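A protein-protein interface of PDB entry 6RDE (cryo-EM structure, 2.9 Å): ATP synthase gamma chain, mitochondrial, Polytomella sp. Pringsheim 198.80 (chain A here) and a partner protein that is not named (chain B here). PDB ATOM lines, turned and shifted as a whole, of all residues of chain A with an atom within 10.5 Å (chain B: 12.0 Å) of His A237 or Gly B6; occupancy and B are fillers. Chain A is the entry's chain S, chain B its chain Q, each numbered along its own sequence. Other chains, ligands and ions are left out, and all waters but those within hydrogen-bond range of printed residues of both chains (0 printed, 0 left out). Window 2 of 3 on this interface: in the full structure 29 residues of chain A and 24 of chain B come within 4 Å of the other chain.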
ATOM      1  N   ASP A 214      33.069   3.937  19.687  1.00  0.00           N
ATOM      2  CA  ASP A 214      32.480   4.927  20.575  1.00  0.00           C
ATOM      3  C   ASP A 214      32.438   4.438  22.009  1.00  0.00           C
ATOM      4  O   ASP A 214      31.919   5.135  22.886  1.00  0.00           O
ATOM      5  CB  ASP A 214      31.076   5.323  20.093  1.00  0.00           C
ATOM      6  CG  ASP A 214      30.205   4.127  19.763  1.00  0.00           C
ATOM      7  OD1 ASP A 214      30.469   3.474  18.735  1.00  0.00           O
ATOM      8  OD2 ASP A 214      29.253   3.843  20.519  1.00  0.00           O
ATOM      9  N   ASP A 232      37.030  15.950   8.738  1.00  0.00           N
ATOM     10  CA  ASP A 232      35.655  16.242   8.365  1.00  0.00           C
ATOM     11  C   ASP A 232      35.019  15.014   7.735  1.00  0.00           C
ATOM     12  O   ASP A 232      35.343  14.644   6.606  1.00  0.00           O
ATOM     13  CB  ASP A 232      35.595  17.459   7.457  1.00  0.00           C
ATOM     14  CG  ASP A 232      35.747  18.726   8.244  1.00  0.00           C
ATOM     15  OD1 ASP A 232      34.795  19.048   8.977  1.00  0.00           O
ATOM     16  OD2 ASP A 232      36.801  19.383   8.157  1.00  0.00           O
ATOM     17  N   ILE A 233      34.094  14.410   8.474  1.00  0.00           N
ATOM     18  CA  ILE A 233      33.528  13.111   8.143  1.00  0.00           C
ATOM     19  C   ILE A 233      32.613  13.243   6.936  1.00  0.00           C
ATOM     20  O   ILE A 233      31.603  13.952   6.974  1.00  0.00           O
ATOM     21  CB  ILE A 233      32.768  12.538   9.343  1.00  0.00           C
ATOM     22  CG1 ILE A 233      33.696  12.366  10.544  1.00  0.00           C
ATOM     23  CG2 ILE A 233      32.107  11.255   8.965  1.00  0.00           C
ATOM     24  CD1 ILE A 233      34.885  11.494  10.285  1.00  0.00           C
ATOM     25  N   GLU A 234      32.954  12.541   5.864  1.00  0.00           N
ATOM     26  CA  GLU A 234      32.170  12.513   4.636  1.00  0.00           C
ATOM     27  C   GLU A 234      31.395  11.205   4.545  1.00  0.00           C
ATOM     28  O   GLU A 234      31.328  10.557   3.507  1.00  0.00           O
ATOM     29  CB  GLU A 234      33.107  12.728   3.444  1.00  0.00           C
ATOM     30  CG  GLU A 234      32.521  13.244   2.114  1.00  0.00           C
ATOM     31  CD  GLU A 234      32.223  12.152   1.110  1.00  0.00           C
ATOM     32  OE1 GLU A 234      32.887  11.108   1.150  1.00  0.00           O
ATOM     33  OE2 GLU A 234      31.328  12.328   0.272  1.00  0.00           O
ATOM     34  N   ALA A 235      30.833  10.756   5.659  1.00  0.00           N
ATOM     35  CA  ALA A 235      30.025   9.552   5.655  1.00  0.00           C
ATOM     36  C   ALA A 235      28.568   9.900   5.386  1.00  0.00           C
ATOM     37  O   ALA A 235      28.192  11.066   5.283  1.00  0.00           O
ATOM     38  CB  ALA A 235      30.163   8.807   6.977  1.00  0.00           C
ATOM     39  N   SER A 236      27.737   8.872   5.263  1.00  0.00           N
ATOM     40  CA  SER A 236      26.301   9.085   5.153  1.00  0.00           C
ATOM     41  C   SER A 236      25.669   9.307   6.515  1.00  0.00           C
ATOM     42  O   SER A 236      24.725  10.090   6.643  1.00  0.00           O
ATOM     43  CB  SER A 236      25.636   7.897   4.458  1.00  0.00           C
ATOM     44  OG  SER A 236      26.020   6.677   5.059  1.00  0.00           O
ATOM     45  N   HIS A 237      26.174   8.636   7.535  1.00  0.00           N
ATOM     46  CA  HIS A 237      25.694   8.799   8.891  1.00  0.00           C
ATOM     47  C   HIS A 237      26.792   9.439   9.732  1.00  0.00           C
ATOM     48  O   HIS A 237      27.845   9.825   9.221  1.00  0.00           O
ATOM     49  CB  HIS A 237      25.209   7.452   9.407  1.00  0.00           C
ATOM     50  CG  HIS A 237      24.037   6.921   8.643  1.00  0.00           C
ATOM     51  ND1 HIS A 237      24.145   6.430   7.361  1.00  0.00           N
ATOM     52  CD2 HIS A 237      22.729   6.819   8.973  1.00  0.00           C
ATOM     53  CE1 HIS A 237      22.957   6.039   6.938  1.00  0.00           C
ATOM     54  NE2 HIS A 237      22.081   6.265   7.896  1.00  0.00           N
ATOM     55  N   GLU A 238      26.545   9.591  11.028  1.00  0.00           N
ATOM     56  CA  GLU A 238      27.424  10.423  11.835  1.00  0.00           C
ATOM     57  C   GLU A 238      28.654   9.632  12.286  1.00  0.00           C
ATOM     58  O   GLU A 238      28.845   8.468  11.929  1.00  0.00           O
ATOM     59  CB  GLU A 238      26.638  11.049  12.988  1.00  0.00           C
ATOM     60  CG  GLU A 238      26.005  10.091  13.963  1.00  0.00           C
ATOM     61  CD  GLU A 238      26.870   9.848  15.176  1.00  0.00           C
ATOM     62  OE1 GLU A 238      27.777  10.667  15.428  1.00  0.00           O
ATOM     63  OE2 GLU A 238      26.626   8.852  15.890  1.00  0.00           O
ATOM     64  N   ARG A 239      29.503  10.301  13.072  1.00  0.00           N
ATOM     65  CA  ARG A 239      30.881   9.865  13.286  1.00  0.00           C
ATOM     66  C   ARG A 239      30.984   8.552  14.053  1.00  0.00           C
ATOM     67  O   ARG A 239      31.931   7.789  13.840  1.00  0.00           O
ATOM     68  CB  ARG A 239      31.662  10.965  14.006  1.00  0.00           C
ATOM     69  CG  ARG A 239      33.158  10.746  14.019  1.00  0.00           C
ATOM     70  CD  ARG A 239      33.925  11.977  14.443  1.00  0.00           C
ATOM     71  NE  ARG A 239      34.104  12.092  15.879  1.00  0.00           N
ATOM     72  CZ  ARG A 239      34.564  13.188  16.462  1.00  0.00           C
ATOM     73  NH1 ARG A 239      34.887  14.233  15.718  1.00  0.00           N
ATOM     74  NH2 ARG A 239      34.712  13.246  17.776  1.00  0.00           N
ATOM     75  N   SER A 240      30.036   8.257  14.937  1.00  0.00           N
ATOM     76  CA  SER A 240      30.124   7.000  15.668  1.00  0.00           C
ATOM     77  C   SER A 240      29.806   5.798  14.798  1.00  0.00           C
ATOM     78  O   SER A 240      30.235   4.689  15.127  1.00  0.00           O
ATOM     79  CB  SER A 240      29.183   7.023  16.864  1.00  0.00           C
ATOM     80  OG  SER A 240      27.840   6.976  16.429  1.00  0.00           O
ATOM     81  N   ASP A 241      29.077   5.986  13.702  1.00  0.00           N
ATOM     82  CA  ASP A 241      28.818   4.902  12.771  1.00  0.00           C
ATOM     83  C   ASP A 241      29.906   4.754  11.726  1.00  0.00           C
ATOM     84  O   ASP A 241      30.097   3.653  11.206  1.00  0.00           O
ATOM     85  CB  ASP A 241      27.472   5.102  12.069  1.00  0.00           C
ATOM     86  CG  ASP A 241      26.290   4.846  12.985  1.00  0.00           C
ATOM     87  OD1 ASP A 241      26.431   4.055  13.938  1.00  0.00           O
ATOM     88  OD2 ASP A 241      25.209   5.424  12.749  1.00  0.00           O
ATOM     89  N   VAL A 242      30.628   5.829  11.402  1.00  0.00           N
ATOM     90  CA  VAL A 242      31.751   5.678  10.488  1.00  0.00           C
ATOM     91  C   VAL A 242      32.948   5.120  11.238  1.00  0.00           C
ATOM     92  O   VAL A 242      33.786   4.439  10.650  1.00  0.00           O
ATOM     93  CB  VAL A 242      32.066   7.008   9.765  1.00  0.00           C
ATOM     94  CG1 VAL A 242      32.737   8.003  10.659  1.00  0.00           C
ATOM     95  CG2 VAL A 242      32.919   6.783   8.556  1.00  0.00           C
ATOM     96  N   LEU A 243      33.026   5.340  12.552  1.00  0.00           N
ATOM     97  CA  LEU A 243      34.109   4.764  13.336  1.00  0.00           C
ATOM     98  C   LEU A 243      33.856   3.307  13.646  1.00  0.00           C
ATOM     99  O   LEU A 243      34.799   2.560  13.912  1.00  0.00           O
ATOM    100  CB  LEU A 243      34.292   5.529  14.634  1.00  0.00           C
ATOM    101  CG  LEU A 243      35.468   6.490  14.713  1.00  0.00           C
ATOM    102  CD1 LEU A 243      35.274   7.665  13.802  1.00  0.00           C
ATOM    103  CD2 LEU A 243      35.606   6.935  16.139  1.00  0.00           C
ATOM    104  N   ARG A 244      32.593   2.898  13.658  1.00  0.00           N
ATOM    105  CA  ARG A 244      32.281   1.487  13.808  1.00  0.00           C
ATOM    106  C   ARG A 244      32.700   0.709  12.570  1.00  0.00           C
ATOM    107  O   ARG A 244      33.317  -0.351  12.683  1.00  0.00           O
ATOM    108  CB  ARG A 244      30.795   1.315  14.084  1.00  0.00           C
ATOM    109  CG  ARG A 244      30.342  -0.108  14.153  1.00  0.00           C
ATOM    110  CD  ARG A 244      30.861  -0.774  15.399  1.00  0.00           C
ATOM    111  NE  ARG A 244      30.359  -0.115  16.595  1.00  0.00           N
ATOM    112  CZ  ARG A 244      30.439  -0.627  17.815  1.00  0.00           C
ATOM    113  NH1 ARG A 244      29.954   0.050  18.845  1.00  0.00           N
ATOM    114  NH2 ARG A 244      30.996  -1.815  18.003  1.00  0.00           N
ATOM    115  N   ASP A 245      32.408   1.242  11.381  1.00  0.00           N
ATOM    116  CA  ASP A 245      32.862   0.625  10.141  1.00  0.00           C
ATOM    117  C   ASP A 245      34.368   0.687   9.979  1.00  0.00           C
ATOM    118  O   ASP A 245      34.942  -0.159   9.293  1.00  0.00           O
ATOM    119  CB  ASP A 245      32.216   1.302   8.937  1.00  0.00           C
ATOM    120  CG  ASP A 245      30.714   1.239   8.966  1.00  0.00           C
ATOM    121  OD1 ASP A 245      30.173   0.173   9.320  1.00  0.00           O
ATOM    122  OD2 ASP A 245      30.064   2.251   8.628  1.00  0.00           O
ATOM    123  N   ALA B   3      15.688  -2.417  15.773  1.00  0.00           N
ATOM    124  CA  ALA B   3      16.593  -1.992  16.839  1.00  0.00           C
ATOM    125  C   ALA B   3      17.703  -0.985  16.433  1.00  0.00           C
ATOM    126  O   ALA B   3      17.673   0.143  16.927  1.00  0.00           O
ATOM    127  CB  ALA B   3      17.217  -3.226  17.518  1.00  0.00           C
ATOM    128  N   PRO B   4      18.656  -1.343  15.559  1.00  0.00           N
ATOM    129  CA  PRO B   4      19.918  -0.597  15.532  1.00  0.00           C
ATOM    130  C   PRO B   4      19.817   0.708  14.753  1.00  0.00           C
ATOM    131  O   PRO B   4      18.808   1.027  14.125  1.00  0.00           O
ATOM    132  CB  PRO B   4      20.886  -1.566  14.842  1.00  0.00           C
ATOM    133  CG  PRO B   4      20.011  -2.600  14.154  1.00  0.00           C
ATOM    134  CD  PRO B   4      18.585  -2.203  14.359  1.00  0.00           C
ATOM    135  N   SER B   5      20.897   1.478  14.826  1.00  0.00           N
ATOM    136  CA  SER B   5      21.022   2.744  14.117  1.00  0.00           C
ATOM    137  C   SER B   5      22.299   2.711  13.290  1.00  0.00           C
ATOM    138  O   SER B   5      23.362   2.343  13.803  1.00  0.00           O
ATOM    139  CB  SER B   5      21.039   3.916  15.099  1.00  0.00           C
ATOM    140  OG  SER B   5      21.210   5.157  14.433  1.00  0.00           O
ATOM    141  N   GLY B   6      22.196   3.077  12.016  1.00  0.00           N
ATOM    142  CA  GLY B   6      23.356   3.181  11.167  1.00  0.00           C
ATOM    143  C   GLY B   6      23.006   3.142   9.697  1.00  0.00           C
ATOM    144  O   GLY B   6      21.906   3.519   9.293  1.00  0.00           O
ATOM    145  N   PRO B   7      23.939   2.684   8.867  1.00  0.00           N
ATOM    146  CA  PRO B   7      23.648   2.535   7.437  1.00  0.00           C
ATOM    147  C   PRO B   7      22.737   1.364   7.121  1.00  0.00           C
ATOM    148  O   PRO B   7      22.260   0.674   8.024  1.00  0.00           O
ATOM    149  CB  PRO B   7      25.036   2.334   6.826  1.00  0.00           C
ATOM    150  CG  PRO B   7      25.960   2.951   7.797  1.00  0.00           C
ATOM    151  CD  PRO B   7      25.383   2.662   9.128  1.00  0.00           C
ATOM    152  N   PHE B   8      22.501   1.118   5.832  1.00  0.00           N
ATOM    153  CA  PHE B   8      21.546   0.093   5.437  1.00  0.00           C
ATOM    154  C   PHE B   8      22.060  -1.317   5.666  1.00  0.00           C
ATOM    155  O   PHE B   8      21.253  -2.241   5.798  1.00  0.00           O
ATOM    156  CB  PHE B   8      21.151   0.264   3.974  1.00  0.00           C
ATOM    157  CG  PHE B   8      22.219  -0.124   2.994  1.00  0.00           C
ATOM    158  CD1 PHE B   8      22.160  -1.336   2.325  1.00  0.00           C
ATOM    159  CD2 PHE B   8      23.252   0.741   2.704  1.00  0.00           C
ATOM    160  CE1 PHE B   8      23.127  -1.684   1.422  1.00  0.00           C
ATOM    161  CE2 PHE B   8      24.221   0.395   1.796  1.00  0.00           C
ATOM    162  CZ  PHE B   8      24.157  -0.818   1.156  1.00  0.00           C
ATOM    163  N   TYR B   9      23.374  -1.514   5.698  1.00  0.00           N
ATOM    164  CA  TYR B   9      23.888  -2.808   6.110  1.00  0.00           C
ATOM    165  C   TYR B   9      23.847  -2.970   7.621  1.00  0.00           C
ATOM    166  O   TYR B   9      23.630  -4.079   8.113  1.00  0.00           O
ATOM    167  CB  TYR B   9      25.310  -3.012   5.587  1.00  0.00           C
ATOM    168  CG  TYR B   9      26.264  -1.862   5.803  1.00  0.00           C
ATOM    169  CD1 TYR B   9      26.478  -0.922   4.809  1.00  0.00           C
ATOM    170  CD2 TYR B   9      26.979  -1.740   6.982  1.00  0.00           C
ATOM    171  CE1 TYR B   9      27.355   0.117   4.994  1.00  0.00           C
ATOM    172  CE2 TYR B   9      27.855  -0.702   7.177  1.00  0.00           C
ATOM    173  CZ  TYR B   9      28.040   0.221   6.179  1.00  0.00           C
ATOM    174  OH  TYR B   9      28.917   1.254   6.365  1.00  0.00           O
ATOM    175  N   ARG B  10      24.024  -1.879   8.365  1.00  0.00           N
ATOM    176  CA  ARG B  10      24.097  -1.969   9.818  1.00  0.00           C
ATOM    177  C   ARG B  10      22.727  -2.192  10.431  1.00  0.00           C
ATOM    178  O   ARG B  10      22.621  -2.829  11.484  1.00  0.00           O
ATOM    179  CB  ARG B  10      24.740  -0.704  10.380  1.00  0.00           C
ATOM    180  CG  ARG B  10      25.093  -0.734  11.851  1.00  0.00           C
ATOM    181  CD  ARG B  10      26.170  -1.750  12.146  1.00  0.00           C
ATOM    182  NE  ARG B  10      27.458  -1.391  11.565  1.00  0.00           N
ATOM    183  CZ  ARG B  10      28.583  -2.056  11.794  1.00  0.00           C
ATOM    184  NH1 ARG B  10      28.576  -3.109  12.591  1.00  0.00           N
ATOM    185  NH2 ARG B  10      29.717  -1.668  11.234  1.00  0.00           N
ATOM    186  N   VAL B  11      21.667  -1.692   9.786  1.00  0.00           N
ATOM    187  CA  VAL B  11      20.317  -1.863  10.319  1.00  0.00           C
ATOM    188  C   VAL B  11      19.710  -3.204   9.954  1.00  0.00           C
ATOM    189  O   VAL B  11      18.619  -3.527  10.437  1.00  0.00           O
ATOM    190  CB  VAL B  11      19.348  -0.773   9.830  1.00  0.00           C
ATOM    191  CG1 VAL B  11      19.738   0.590  10.395  1.00  0.00           C
ATOM    192  CG2 VAL B  11      19.285  -0.765   8.321  1.00  0.00           C
ATOM    193  N   ALA B  12      20.378  -3.993   9.115  1.00  0.00           N
ATOM    194  CA  ALA B  12      19.898  -5.313   8.738  1.00  0.00           C
ATOM    195  C   ALA B  12      20.656  -6.441   9.418  1.00  0.00           C
ATOM    196  O   ALA B  12      20.427  -7.608   9.088  1.00  0.00           O
ATOM    197  CB  ALA B  12      19.974  -5.494   7.231  1.00  0.00           C
ATOM    198  N   GLY B  13      21.544  -6.130  10.358  1.00  0.00           N
ATOM    199  CA  GLY B  13      22.316  -7.169  11.004  1.00  0.00           C
ATOM    200  C   GLY B  13      23.533  -7.632  10.238  1.00  0.00           C
ATOM    201  O   GLY B  13      23.963  -8.775  10.423  1.00  0.00           O
ATOM    202  N   MET B  14      24.088  -6.786   9.375  1.00  0.00           N
ATOM    203  CA  MET B  14      25.273  -7.100   8.588  1.00  0.00           C
ATOM    204  C   MET B  14      26.398  -6.150   8.976  1.00  0.00           C
ATOM    205  O   MET B  14      26.181  -4.941   9.086  1.00  0.00           O
ATOM    206  CB  MET B  14      24.958  -6.987   7.099  1.00  0.00           C
ATOM    207  CG  MET B  14      26.135  -7.150   6.185  1.00  0.00           C
ATOM    208  SD  MET B  14      25.705  -6.687   4.511  1.00  0.00           S
ATOM    209  CE  MET B  14      24.306  -7.750   4.245  1.00  0.00           C
ATOM    210  N   SER B  15      27.593  -6.690   9.187  1.00  0.00           N
ATOM    211  CA  SER B  15      28.721  -5.875   9.611  1.00  0.00           C
ATOM    212  C   SER B  15      29.283  -5.091   8.429  1.00  0.00           C
ATOM    213  O   SER B  15      28.819  -5.207   7.295  1.00  0.00           O
ATOM    214  CB  SER B  15      29.796  -6.749  10.248  1.00  0.00           C
ATOM    215  OG  SER B  15      30.328  -7.662   9.307  1.00  0.00           O
ATOM    216  N   TYR B  16      30.303  -4.275   8.693  1.00  0.00           N
ATOM    217  CA  TYR B  16      30.955  -3.585   7.589  1.00  0.00           C
ATOM    218  C   TYR B  16      31.821  -4.538   6.787  1.00  0.00           C
ATOM    219  O   TYR B  16      31.896  -4.434   5.558  1.00  0.00           O
ATOM    220  CB  TYR B  16      31.807  -2.429   8.083  1.00  0.00           C
ATOM    221  CG  TYR B  16      32.424  -1.714   6.915  1.00  0.00           C
ATOM    222  CD1 TYR B  16      31.626  -1.036   6.011  1.00  0.00           C
ATOM    223  CD2 TYR B  16      33.790  -1.754   6.683  1.00  0.00           C
ATOM    224  CE1 TYR B  16      32.156  -0.399   4.932  1.00  0.00           C
ATOM    225  CE2 TYR B  16      34.333  -1.113   5.590  1.00  0.00           C
ATOM    226  CZ  TYR B  16      33.504  -0.438   4.719  1.00  0.00           C
ATOM    227  OH  TYR B  16      34.015   0.212   3.628  1.00  0.00           O
ATOM    228  N   TYR B  19      29.637  -6.475   4.579  1.00  0.00           N
ATOM    229  CA  TYR B  19      29.110  -5.666   3.491  1.00  0.00           C
ATOM    230  C   TYR B  19      30.181  -5.387   2.453  1.00  0.00           C
ATOM    231  O   TYR B  19      29.935  -5.499   1.249  1.00  0.00           O
ATOM    232  CB  TYR B  19      28.544  -4.354   4.037  1.00  0.00           C
ATOM    233  CG  TYR B  19      28.481  -3.238   3.019  1.00  0.00           C
ATOM    234  CD1 TYR B  19      29.397  -2.189   3.047  1.00  0.00           C
ATOM    235  CD2 TYR B  19      27.500  -3.228   2.039  1.00  0.00           C
ATOM    236  CE1 TYR B  19      29.349  -1.184   2.124  1.00  0.00           C
ATOM    237  CE2 TYR B  19      27.439  -2.214   1.115  1.00  0.00           C
ATOM    238  CZ  TYR B  19      28.366  -1.195   1.162  1.00  0.00           C
ATOM    239  OH  TYR B  19      28.307  -0.180   0.235  1.00  0.00           O
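O of Gly B6 is in hydrogen-bond range of NE2 of His A237 (3.1 Å).
OD2 of Asp A245 sits at hydrogen-bond distance from OH of Tyr B9, at 2.7 Å.
The guanidinium group (NH2) of Arg B10 is in salt-bridge range of the side-chain carboxylate (OD1) of Asp A245, at 2.7 Å.
The backbone carbonyl oxygen of Tyr B9 is in hydrogen-bond range of the backbone NH of Met B14 (3.0 Å).
The side-chain carboxylate (OD1) of Asp A214 is in salt-bridge range of the guanidinium group (NH1) of Arg A244, 3.5 Å away.
OG of Ser A236 sits at hydrogen-bond distance from ND1 of His A237.
Among the printed residues, pairs that only touch across the chains: Asp A245 with Tyr B16, Asp A241 with Gly B6, Arg A244 with Arg B10, Asp A241 with Ser B5 and His A237 with Pro B7.
His A237 touches just these residues of chain B: Gly B6 and Pro B7.
Gly B6 touches two residues of chain A.
No residue of chain B comes within 4 Å of Ile A233.
No residue of chain B comes within 4 Å of Ala A235.
No residue of chain B comes within 4 Å of Ser A236.
Of chain A, only Asp A241 (3.5 Å) comes within 4 Å of Ser B5.
Of the printed residues of chain A, Tyr B16 touches Asp A245 (3.3 Å).
Of the printed residues of chain A, Arg B10 touches Arg A244 (3.4 Å) and Asp A245 (2.7 Å).
Val B11 touches none of the printed residues of chain A.
Arg A239 touches none of the printed residues of chain B.
The nearest residue of chain B that does not touch His A237 is Phe B8 (5.1 Å).
The nearest printed residue of chain A that does not touch Tyr B9 is Asp A241 (5.5 Å).
Of the 15 printed residues of chain A, 4 touch a printed residue of chain B.
Of the 15 printed residues of chain B, 6 touch a printed residue of chain A.
Among the printed residues, 8 pairs touch across the chains.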
